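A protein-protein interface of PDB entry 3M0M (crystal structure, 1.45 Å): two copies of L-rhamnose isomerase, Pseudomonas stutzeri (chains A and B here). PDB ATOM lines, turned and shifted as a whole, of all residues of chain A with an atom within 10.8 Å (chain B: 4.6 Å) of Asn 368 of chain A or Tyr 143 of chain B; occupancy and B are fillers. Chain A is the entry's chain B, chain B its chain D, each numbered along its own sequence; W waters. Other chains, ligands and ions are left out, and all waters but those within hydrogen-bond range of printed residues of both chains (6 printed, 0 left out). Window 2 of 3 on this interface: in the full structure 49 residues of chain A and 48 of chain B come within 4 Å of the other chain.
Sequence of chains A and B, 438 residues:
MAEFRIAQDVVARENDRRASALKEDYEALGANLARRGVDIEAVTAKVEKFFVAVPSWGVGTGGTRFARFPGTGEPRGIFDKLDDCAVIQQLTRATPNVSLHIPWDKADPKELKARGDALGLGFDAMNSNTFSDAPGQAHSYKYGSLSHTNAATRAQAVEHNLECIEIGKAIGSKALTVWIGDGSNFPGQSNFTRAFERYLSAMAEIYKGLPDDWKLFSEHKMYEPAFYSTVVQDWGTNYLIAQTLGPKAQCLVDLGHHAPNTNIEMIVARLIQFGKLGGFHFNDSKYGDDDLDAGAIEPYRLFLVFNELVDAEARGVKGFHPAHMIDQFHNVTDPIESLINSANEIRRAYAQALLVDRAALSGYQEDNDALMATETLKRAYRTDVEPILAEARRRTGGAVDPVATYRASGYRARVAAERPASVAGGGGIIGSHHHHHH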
ATOM      1  N   ALA A 360      15.677  25.493  -8.873  1.00  0.00           N
ATOM      2  CA  ALA A 360      14.995  25.285  -7.603  1.00  0.00           C
ATOM      3  C   ALA A 360      15.821  24.354  -6.722  1.00  0.00           C
ATOM      4  O   ALA A 360      16.010  24.617  -5.535  1.00  0.00           O
ATOM      5  CB  ALA A 360      13.614  24.689  -7.843  1.00  0.00           C
ATOM      6  N   LEU A 361      16.322  23.273  -7.313  1.00  0.00           N
ATOM      7  CA  LEU A 361      17.122  22.310  -6.568  1.00  0.00           C
ATOM      8  C   LEU A 361      18.346  22.981  -5.957  1.00  0.00           C
ATOM      9  O   LEU A 361      18.649  22.784  -4.782  1.00  0.00           O
ATOM     10  CB  LEU A 361      17.571  21.168  -7.478  1.00  0.00           C
ATOM     11  CG  LEU A 361      18.364  20.049  -6.794  1.00  0.00           C
ATOM     12  CD1 LEU A 361      17.539  19.429  -5.668  1.00  0.00           C
ATOM     13  CD2 LEU A 361      18.742  19.000  -7.819  1.00  0.00           C
ATOM     14  N   SER A 362      19.050  23.771  -6.758  1.00  0.00           N
ATOM     15  CA  SER A 362      20.238  24.468  -6.276  1.00  0.00           C
ATOM     16  C   SER A 362      19.908  25.340  -5.067  1.00  0.00           C
ATOM     17  O   SER A 362      20.657  25.376  -4.088  1.00  0.00           O
ATOM     18  CB  SER A 362      20.829  25.337  -7.390  1.00  0.00           C
ATOM     19  OG  SER A 362      21.316  24.531  -8.451  1.00  0.00           O
ATOM     20  N   GLY A 363      18.783  26.042  -5.139  1.00  0.00           N
ATOM     21  CA  GLY A 363      18.383  26.898  -4.039  1.00  0.00           C
ATOM     22  C   GLY A 363      18.142  26.110  -2.766  1.00  0.00           C
ATOM     23  O   GLY A 363      18.608  26.488  -1.692  1.00  0.00           O
ATOM     24  N   TYR A 364      17.411  25.005  -2.883  1.00  0.00           N
ATOM     25  CA  TYR A 364      17.115  24.177  -1.723  1.00  0.00           C
ATOM     26  C   TYR A 364      18.367  23.529  -1.155  1.00  0.00           C
ATOM     27  O   TYR A 364      18.442  23.253   0.041  1.00  0.00           O
ATOM     28  CB  TYR A 364      16.079  23.108  -2.080  1.00  0.00           C
ATOM     29  CG  TYR A 364      14.713  23.671  -2.397  1.00  0.00           C
ATOM     30  CD1 TYR A 364      14.106  24.603  -1.549  1.00  0.00           C
ATOM     31  CD2 TYR A 364      14.014  23.260  -3.529  1.00  0.00           C
ATOM     32  CE1 TYR A 364      12.837  25.107  -1.824  1.00  0.00           C
ATOM     33  CE2 TYR A 364      12.744  23.756  -3.810  1.00  0.00           C
ATOM     34  CZ  TYR A 364      12.162  24.679  -2.954  1.00  0.00           C
ATOM     35  OH  TYR A 364      10.903  25.166  -3.230  1.00  0.00           O
ATOM     36  N   GLN A 365      19.354  23.283  -2.011  1.00  0.00           N
ATOM     37  CA  GLN A 365      20.599  22.689  -1.546  1.00  0.00           C
ATOM     38  C   GLN A 365      21.397  23.724  -0.763  1.00  0.00           C
ATOM     39  O   GLN A 365      21.889  23.446   0.330  1.00  0.00           O
ATOM     40  CB  GLN A 365      21.417  22.170  -2.733  1.00  0.00           C
ATOM     41  CG  GLN A 365      20.697  21.071  -3.504  1.00  0.00           C
ATOM     42  CD  GLN A 365      21.490  20.541  -4.685  1.00  0.00           C
ATOM     43  OE1 GLN A 365      22.193  21.284  -5.364  1.00  0.00           O
ATOM     44  NE2 GLN A 365      21.360  19.246  -4.947  1.00  0.00           N
ATOM     45  N   GLU A 366      21.510  24.926  -1.315  1.00  0.00           N
ATOM     46  CA  GLU A 366      22.254  25.981  -0.641  1.00  0.00           C
ATOM     47  C   GLU A 366      21.648  26.346   0.706  1.00  0.00           C
ATOM     48  O   GLU A 366      22.375  26.622   1.658  1.00  0.00           O
ATOM     49  CB  GLU A 366      22.331  27.230  -1.524  1.00  0.00           C
ATOM     50  CG  GLU A 366      23.233  27.073  -2.735  1.00  0.00           C
ATOM     51  CD  GLU A 366      24.632  26.619  -2.359  1.00  0.00           C
ATOM     52  OE1 GLU A 366      25.269  27.283  -1.513  1.00  0.00           O
ATOM     53  OE2 GLU A 366      25.098  25.600  -2.911  1.00  0.00           O
ATOM     54  N   ASP A 367      20.320  26.330   0.793  1.00  0.00           N
ATOM     55  CA  ASP A 367      19.644  26.682   2.037  1.00  0.00           C
ATOM     56  C   ASP A 367      19.410  25.509   2.983  1.00  0.00           C
ATOM     57  O   ASP A 367      18.754  25.654   4.016  1.00  0.00           O
ATOM     58  CB  ASP A 367      18.311  27.368   1.735  1.00  0.00           C
ATOM     59  CG  ASP A 367      18.489  28.674   0.992  1.00  0.00           C
ATOM     60  OD1 ASP A 367      19.350  29.479   1.408  1.00  0.00           O
ATOM     61  OD2 ASP A 367      17.767  28.898  -0.001  1.00  0.00           O
ATOM     62  N   ASN A 368      19.957  24.351   2.632  1.00  0.00           N
ATOM     63  CA  ASN A 368      19.820  23.149   3.444  1.00  0.00           C
ATOM     64  C   ASN A 368      18.373  22.750   3.716  1.00  0.00           C
ATOM     65  O   ASN A 368      18.034  22.282   4.804  1.00  0.00           O
ATOM     66  CB  ASN A 368      20.587  23.309   4.761  1.00  0.00           C
ATOM     67  CG  ASN A 368      22.089  23.359   4.549  1.00  0.00           C
ATOM     68  OD1 ASN A 368      22.755  24.328   4.921  1.00  0.00           O
ATOM     69  ND2 ASN A 368      22.629  22.313   3.937  1.00  0.00           N
ATOM     70  N   ASP A 369      17.524  22.944   2.712  1.00  0.00           N
ATOM     71  CA  ASP A 369      16.119  22.569   2.806  1.00  0.00           C
ATOM     72  C   ASP A 369      16.055  21.170   2.193  1.00  0.00           C
ATOM     73  O   ASP A 369      15.646  20.998   1.044  1.00  0.00           O
ATOM     74  CB  ASP A 369      15.259  23.542   1.999  1.00  0.00           C
ATOM     75  CG  ASP A 369      13.773  23.370   2.263  1.00  0.00           C
ATOM     76  OD1 ASP A 369      13.367  22.299   2.761  1.00  0.00           O
ATOM     77  OD2 ASP A 369      13.005  24.308   1.959  1.00  0.00           O
ATOM     78  N   ALA A 370      16.474  20.179   2.973  1.00  0.00           N
ATOM     79  CA  ALA A 370      16.519  18.790   2.523  1.00  0.00           C
ATOM     80  C   ALA A 370      15.193  18.235   2.025  1.00  0.00           C
ATOM     81  O   ALA A 370      15.152  17.507   1.030  1.00  0.00           O
ATOM     82  CB  ALA A 370      17.062  17.907   3.635  1.00  0.00           C
ATOM     83  N   LEU A 371      14.111  18.572   2.716  1.00  0.00           N
ATOM     84  CA  LEU A 371      12.802  18.081   2.323  1.00  0.00           C
ATOM     85  C   LEU A 371      12.394  18.593   0.950  1.00  0.00           C
ATOM     86  O   LEU A 371      11.961  17.818   0.099  1.00  0.00           O
ATOM     87  CB  LEU A 371      11.754  18.474   3.364  1.00  0.00           C
ATOM     88  CG  LEU A 371      10.344  17.947   3.078  1.00  0.00           C
ATOM     89  CD1 LEU A 371       9.793  17.254   4.308  1.00  0.00           C
ATOM     90  CD2 LEU A 371       9.444  19.101   2.649  1.00  0.00           C
ATOM     91  N   MET A 372      12.529  19.895   0.722  1.00  0.00           N
ATOM     92  CA  MET A 372      12.156  20.432  -0.579  1.00  0.00           C
ATOM     93  C   MET A 372      13.129  20.013  -1.676  1.00  0.00           C
ATOM     94  O   MET A 372      12.736  19.885  -2.831  1.00  0.00           O
ATOM     95  CB  MET A 372      12.035  21.957  -0.529  1.00  0.00           C
ATOM     96  CG  MET A 372      10.762  22.447   0.157  1.00  0.00           C
ATOM     97  SD  MET A 372       9.243  21.697  -0.500  1.00  0.00           S
ATOM     98  CE  MET A 372       9.280  22.264  -2.185  1.00  0.00           C
ATOM     99  N   ALA A 373      14.395  19.806  -1.323  1.00  0.00           N
ATOM    100  CA  ALA A 373      15.371  19.381  -2.319  1.00  0.00           C
ATOM    101  C   ALA A 373      14.999  17.983  -2.818  1.00  0.00           C
ATOM    102  O   ALA A 373      15.001  17.722  -4.020  1.00  0.00           O
ATOM    103  CB  ALA A 373      16.775  19.372  -1.720  1.00  0.00           C
ATOM    104  N   THR A 374      14.662  17.084  -1.901  1.00  0.00           N
ATOM    105  CA  THR A 374      14.302  15.734  -2.312  1.00  0.00           C
ATOM    106  C   THR A 374      12.959  15.720  -3.053  1.00  0.00           C
ATOM    107  O   THR A 374      12.766  14.942  -3.988  1.00  0.00           O
ATOM    108  CB  THR A 374      14.281  14.771  -1.097  1.00  0.00           C
ATOM    109  OG1 THR A 374      14.727  13.473  -1.516  1.00  0.00           O
ATOM    110  CG2 THR A 374      12.884  14.651  -0.511  1.00  0.00           C
ATOM    111  N   TYR B 141      26.504  22.166  13.297  1.00  0.00           N
ATOM    112  CA  TYR B 141      26.989  21.228  12.287  1.00  0.00           C
ATOM    113  C   TYR B 141      25.882  20.272  11.839  1.00  0.00           C
ATOM    114  O   TYR B 141      26.150  19.222  11.257  1.00  0.00           O
ATOM    115  CB  TYR B 141      28.175  20.429  12.832  1.00  0.00           C
ATOM    116  CG  TYR B 141      29.380  21.280  13.158  1.00  0.00           C
ATOM    117  CD1 TYR B 141      29.819  22.268  12.275  1.00  0.00           C
ATOM    118  CD2 TYR B 141      30.099  21.083  14.335  1.00  0.00           C
ATOM    119  CE1 TYR B 141      30.944  23.037  12.555  1.00  0.00           C
ATOM    120  CE2 TYR B 141      31.230  21.846  14.623  1.00  0.00           C
ATOM    121  CZ  TYR B 141      31.644  22.820  13.728  1.00  0.00           C
ATOM    122  OH  TYR B 141      32.756  23.582  14.005  1.00  0.00           O
ATOM    123  N   LYS B 142      24.635  20.646  12.107  1.00  0.00           N
ATOM    124  CA  LYS B 142      23.484  19.827  11.736  1.00  0.00           C
ATOM    125  C   LYS B 142      23.517  19.418  10.264  1.00  0.00           C
ATOM    126  O   LYS B 142      23.268  18.259   9.926  1.00  0.00           O
ATOM    127  CB  LYS B 142      22.191  20.597  12.030  1.00  0.00           C
ATOM    128  CG  LYS B 142      20.907  19.834  11.727  1.00  0.00           C
ATOM    129  CD  LYS B 142      19.693  20.604  12.242  1.00  0.00           C
ATOM    130  CE  LYS B 142      18.418  19.798  12.068  1.00  0.00           C
ATOM    131  NZ  LYS B 142      17.274  20.416  12.805  1.00  0.00           N
ATOM    132  N   TYR B 143      23.841  20.371   9.395  1.00  0.00           N
ATOM    133  CA  TYR B 143      23.883  20.118   7.962  1.00  0.00           C
ATOM    134  C   TYR B 143      25.299  19.992   7.409  1.00  0.00           C
ATOM    135  O   TYR B 143      25.519  20.142   6.206  1.00  0.00           O
ATOM    136  CB  TYR B 143      23.139  21.232   7.223  1.00  0.00           C
ATOM    137  CG  TYR B 143      21.690  21.366   7.631  1.00  0.00           C
ATOM    138  CD1 TYR B 143      20.774  20.344   7.371  1.00  0.00           C
ATOM    139  CD2 TYR B 143      21.234  22.512   8.283  1.00  0.00           C
ATOM    140  CE1 TYR B 143      19.438  20.460   7.749  1.00  0.00           C
ATOM    141  CE2 TYR B 143      19.901  22.639   8.665  1.00  0.00           C
ATOM    142  CZ  TYR B 143      19.011  21.611   8.395  1.00  0.00           C
ATOM    143  OH  TYR B 143      17.691  21.734   8.768  1.00  0.00           O
ATOM    144  N   GLY B 144      26.256  19.709   8.282  1.00  0.00           N
ATOM    145  CA  GLY B 144      27.625  19.564   7.828  1.00  0.00           C
ATOM    146  C   GLY B 144      28.588  20.459   8.570  1.00  0.00           C
ATOM    147  O   GLY B 144      28.189  21.244   9.439  1.00  0.00           O
ATOM    148  N   HIS B 148      29.935  22.145   4.761  1.00  0.00           N
ATOM    149  CA  HIS B 148      28.676  22.872   4.923  1.00  0.00           C
ATOM    150  C   HIS B 148      28.556  23.946   3.835  1.00  0.00           C
ATOM    151  O   HIS B 148      29.557  24.490   3.385  1.00  0.00           O
ATOM    152  CB  HIS B 148      28.650  23.519   6.314  1.00  0.00           C
ATOM    153  CG  HIS B 148      27.288  23.946   6.772  1.00  0.00           C
ATOM    154  ND1 HIS B 148      26.597  24.990   6.195  1.00  0.00           N
ATOM    155  CD2 HIS B 148      26.502  23.479   7.770  1.00  0.00           C
ATOM    156  CE1 HIS B 148      25.441  25.147   6.818  1.00  0.00           C
ATOM    157  NE2 HIS B 148      25.360  24.243   7.778  1.00  0.00           N
ATOM    158  N   THR B 149      27.331  24.247   3.409  1.00  0.00           N
ATOM    159  CA  THR B 149      27.136  25.264   2.378  1.00  0.00           C
ATOM    160  C   THR B 149      27.471  26.671   2.876  1.00  0.00           C
ATOM    161  O   THR B 149      27.810  27.549   2.084  1.00  0.00           O
ATOM    162  CB  THR B 149      25.685  25.271   1.854  1.00  0.00           C
ATOM    163  OG1 THR B 149      24.783  25.456   2.949  1.00  0.00           O
ATOM    164  CG2 THR B 149      25.360  23.961   1.149  1.00  0.00           C
ATOM    165  N   GLN B 189      19.360  16.364  -1.497  1.00  0.00           N
ATOM    166  CA  GLN B 189      19.682  17.268  -0.402  1.00  0.00           C
ATOM    167  C   GLN B 189      21.029  17.931  -0.645  1.00  0.00           C
ATOM    168  O   GLN B 189      21.197  19.127  -0.404  1.00  0.00           O
ATOM    169  CB  GLN B 189      19.706  16.515   0.932  1.00  0.00           C
ATOM    170  CG  GLN B 189      20.268  17.342   2.084  1.00  0.00           C
ATOM    171  CD  GLN B 189      20.273  16.600   3.411  1.00  0.00           C
ATOM    172  OE1 GLN B 189      20.723  17.134   4.431  1.00  0.00           O
ATOM    173  NE2 GLN B 189      19.772  15.372   3.409  1.00  0.00           N
HETATM  174  O   HOH W   1      19.336  20.498   1.219  1.00  0.00           O
HETATM  175  O   HOH W   2      16.150  20.658   6.125  1.00  0.00           O
HETATM  176  O   HOH W   3      23.107  20.998   0.202  1.00  0.00           O
HETATM  177  O   HOH W   4      22.155  19.571   3.785  1.00  0.00           O
HETATM  178  O   HOH W   5      25.329  22.074   4.252  1.00  0.00           O
HETATM  179  O   HOH W   6      27.860  26.831  -0.573  1.00  0.00           O
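No position is printed for both chains. Of the 8 pairs that touch across the chains among the printed residues, none has its exchanged pair printed and touching as well.
Gln 365 of chain A touches Thr 149 of chain B. Gln 189 of chain B touches Gln 365 of chain A. Asn 368 of chain A touches Tyr 143 of chain B (ND2 to CB, 3.5 Å). Asn 368 of chain A touches His 148 of chain B (OD1 to CE1, 3.4 Å). Ala 370 of chain A touches Gln 189 of chain B. CA of Gln 189 of chain B touches CB of Ala 373 of chain A (3.8 Å).
Water W5 lies within hydrogen-bond range of the side-chain amide nitrogen of Asn 368 of chain A (2.7 Å), the backbone carbonyl oxygen of Tyr 143 of chain B (2.8 Å) and the backbone NH of Thr 149 of chain B (3.1 Å). Water W3 lies within hydrogen-bond range of O of Gln 365 of chain A and O of Gln 189 of chain B. Water W6 bridges O of Thr 149 of chain B and OE1 of Glu 366 of chain A. Water W4 bridges ND2 of Asn 368 of chain A (2.8 Å) and OE1 of Gln 189 of chain B (2.9 Å). Water W2 lies within hydrogen-bond range of O of Asn 368 of chain A (2.8 Å), N of Ala 370 of chain A (3.2 Å) and OH of Tyr 143 of chain B (3.2 Å). Water W1 lies within hydrogen-bond range of the backbone carbonyl oxygen of Gln 189 of chain B (2.8 Å), the backbone carbonyl oxygen of Tyr 364 of chain A (3.1 Å), the backbone NH of Ala 370 of chain A (3.4 Å) and the backbone NH of Asp 369 of chain A (3.4 Å).
Asn 368 of chain A touches just these residues of chain B: Tyr 143 (3.5 Å), His 148 (3.4 Å) and Thr 149 (3.0 Å). Tyr 143 of chain B touches one residue of chain A. Gly 144 of chain B touches none of the printed residues of chain A. Printed residues of chain B within 4 Å of Ala 373 of chain A: Gln 189. Of the printed residues of chain B, Ala 370 of chain A touches Gln 189 (3.5 Å). Printed residues of chain B within 4 Å of Glu 366 of chain A: Thr 149 (3.0 Å). The nearest residue of chain A that does not touch Tyr 143 of chain B is Ala 370 of chain A (5.4 Å).
OG1 of Thr 149 of chain B is in hydrogen-bond range of O of Glu 366 of chain A (3.0 Å). The side-chain amide oxygen (OD1) of Asn 368 of chain A sits at hydrogen-bond distance from the side-chain hydroxyl (OG1) of Thr 149 of chain B (3.0 Å).
Of the 15 printed residues of chain A, 5 touch a printed residue of chain B. Hydrophobic or aromatic side chains of chain A within 4 Å of the printed part of chain B: Ala 370 and Ala 373. Printed residues of chain B that touch a printed residue of chain A: Tyr 143, His 148, Thr 149 and Gln 189. Hydrophobic or aromatic side chains of chain B within 4 Å of the printed part of chain A: Tyr 143 and His 148.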
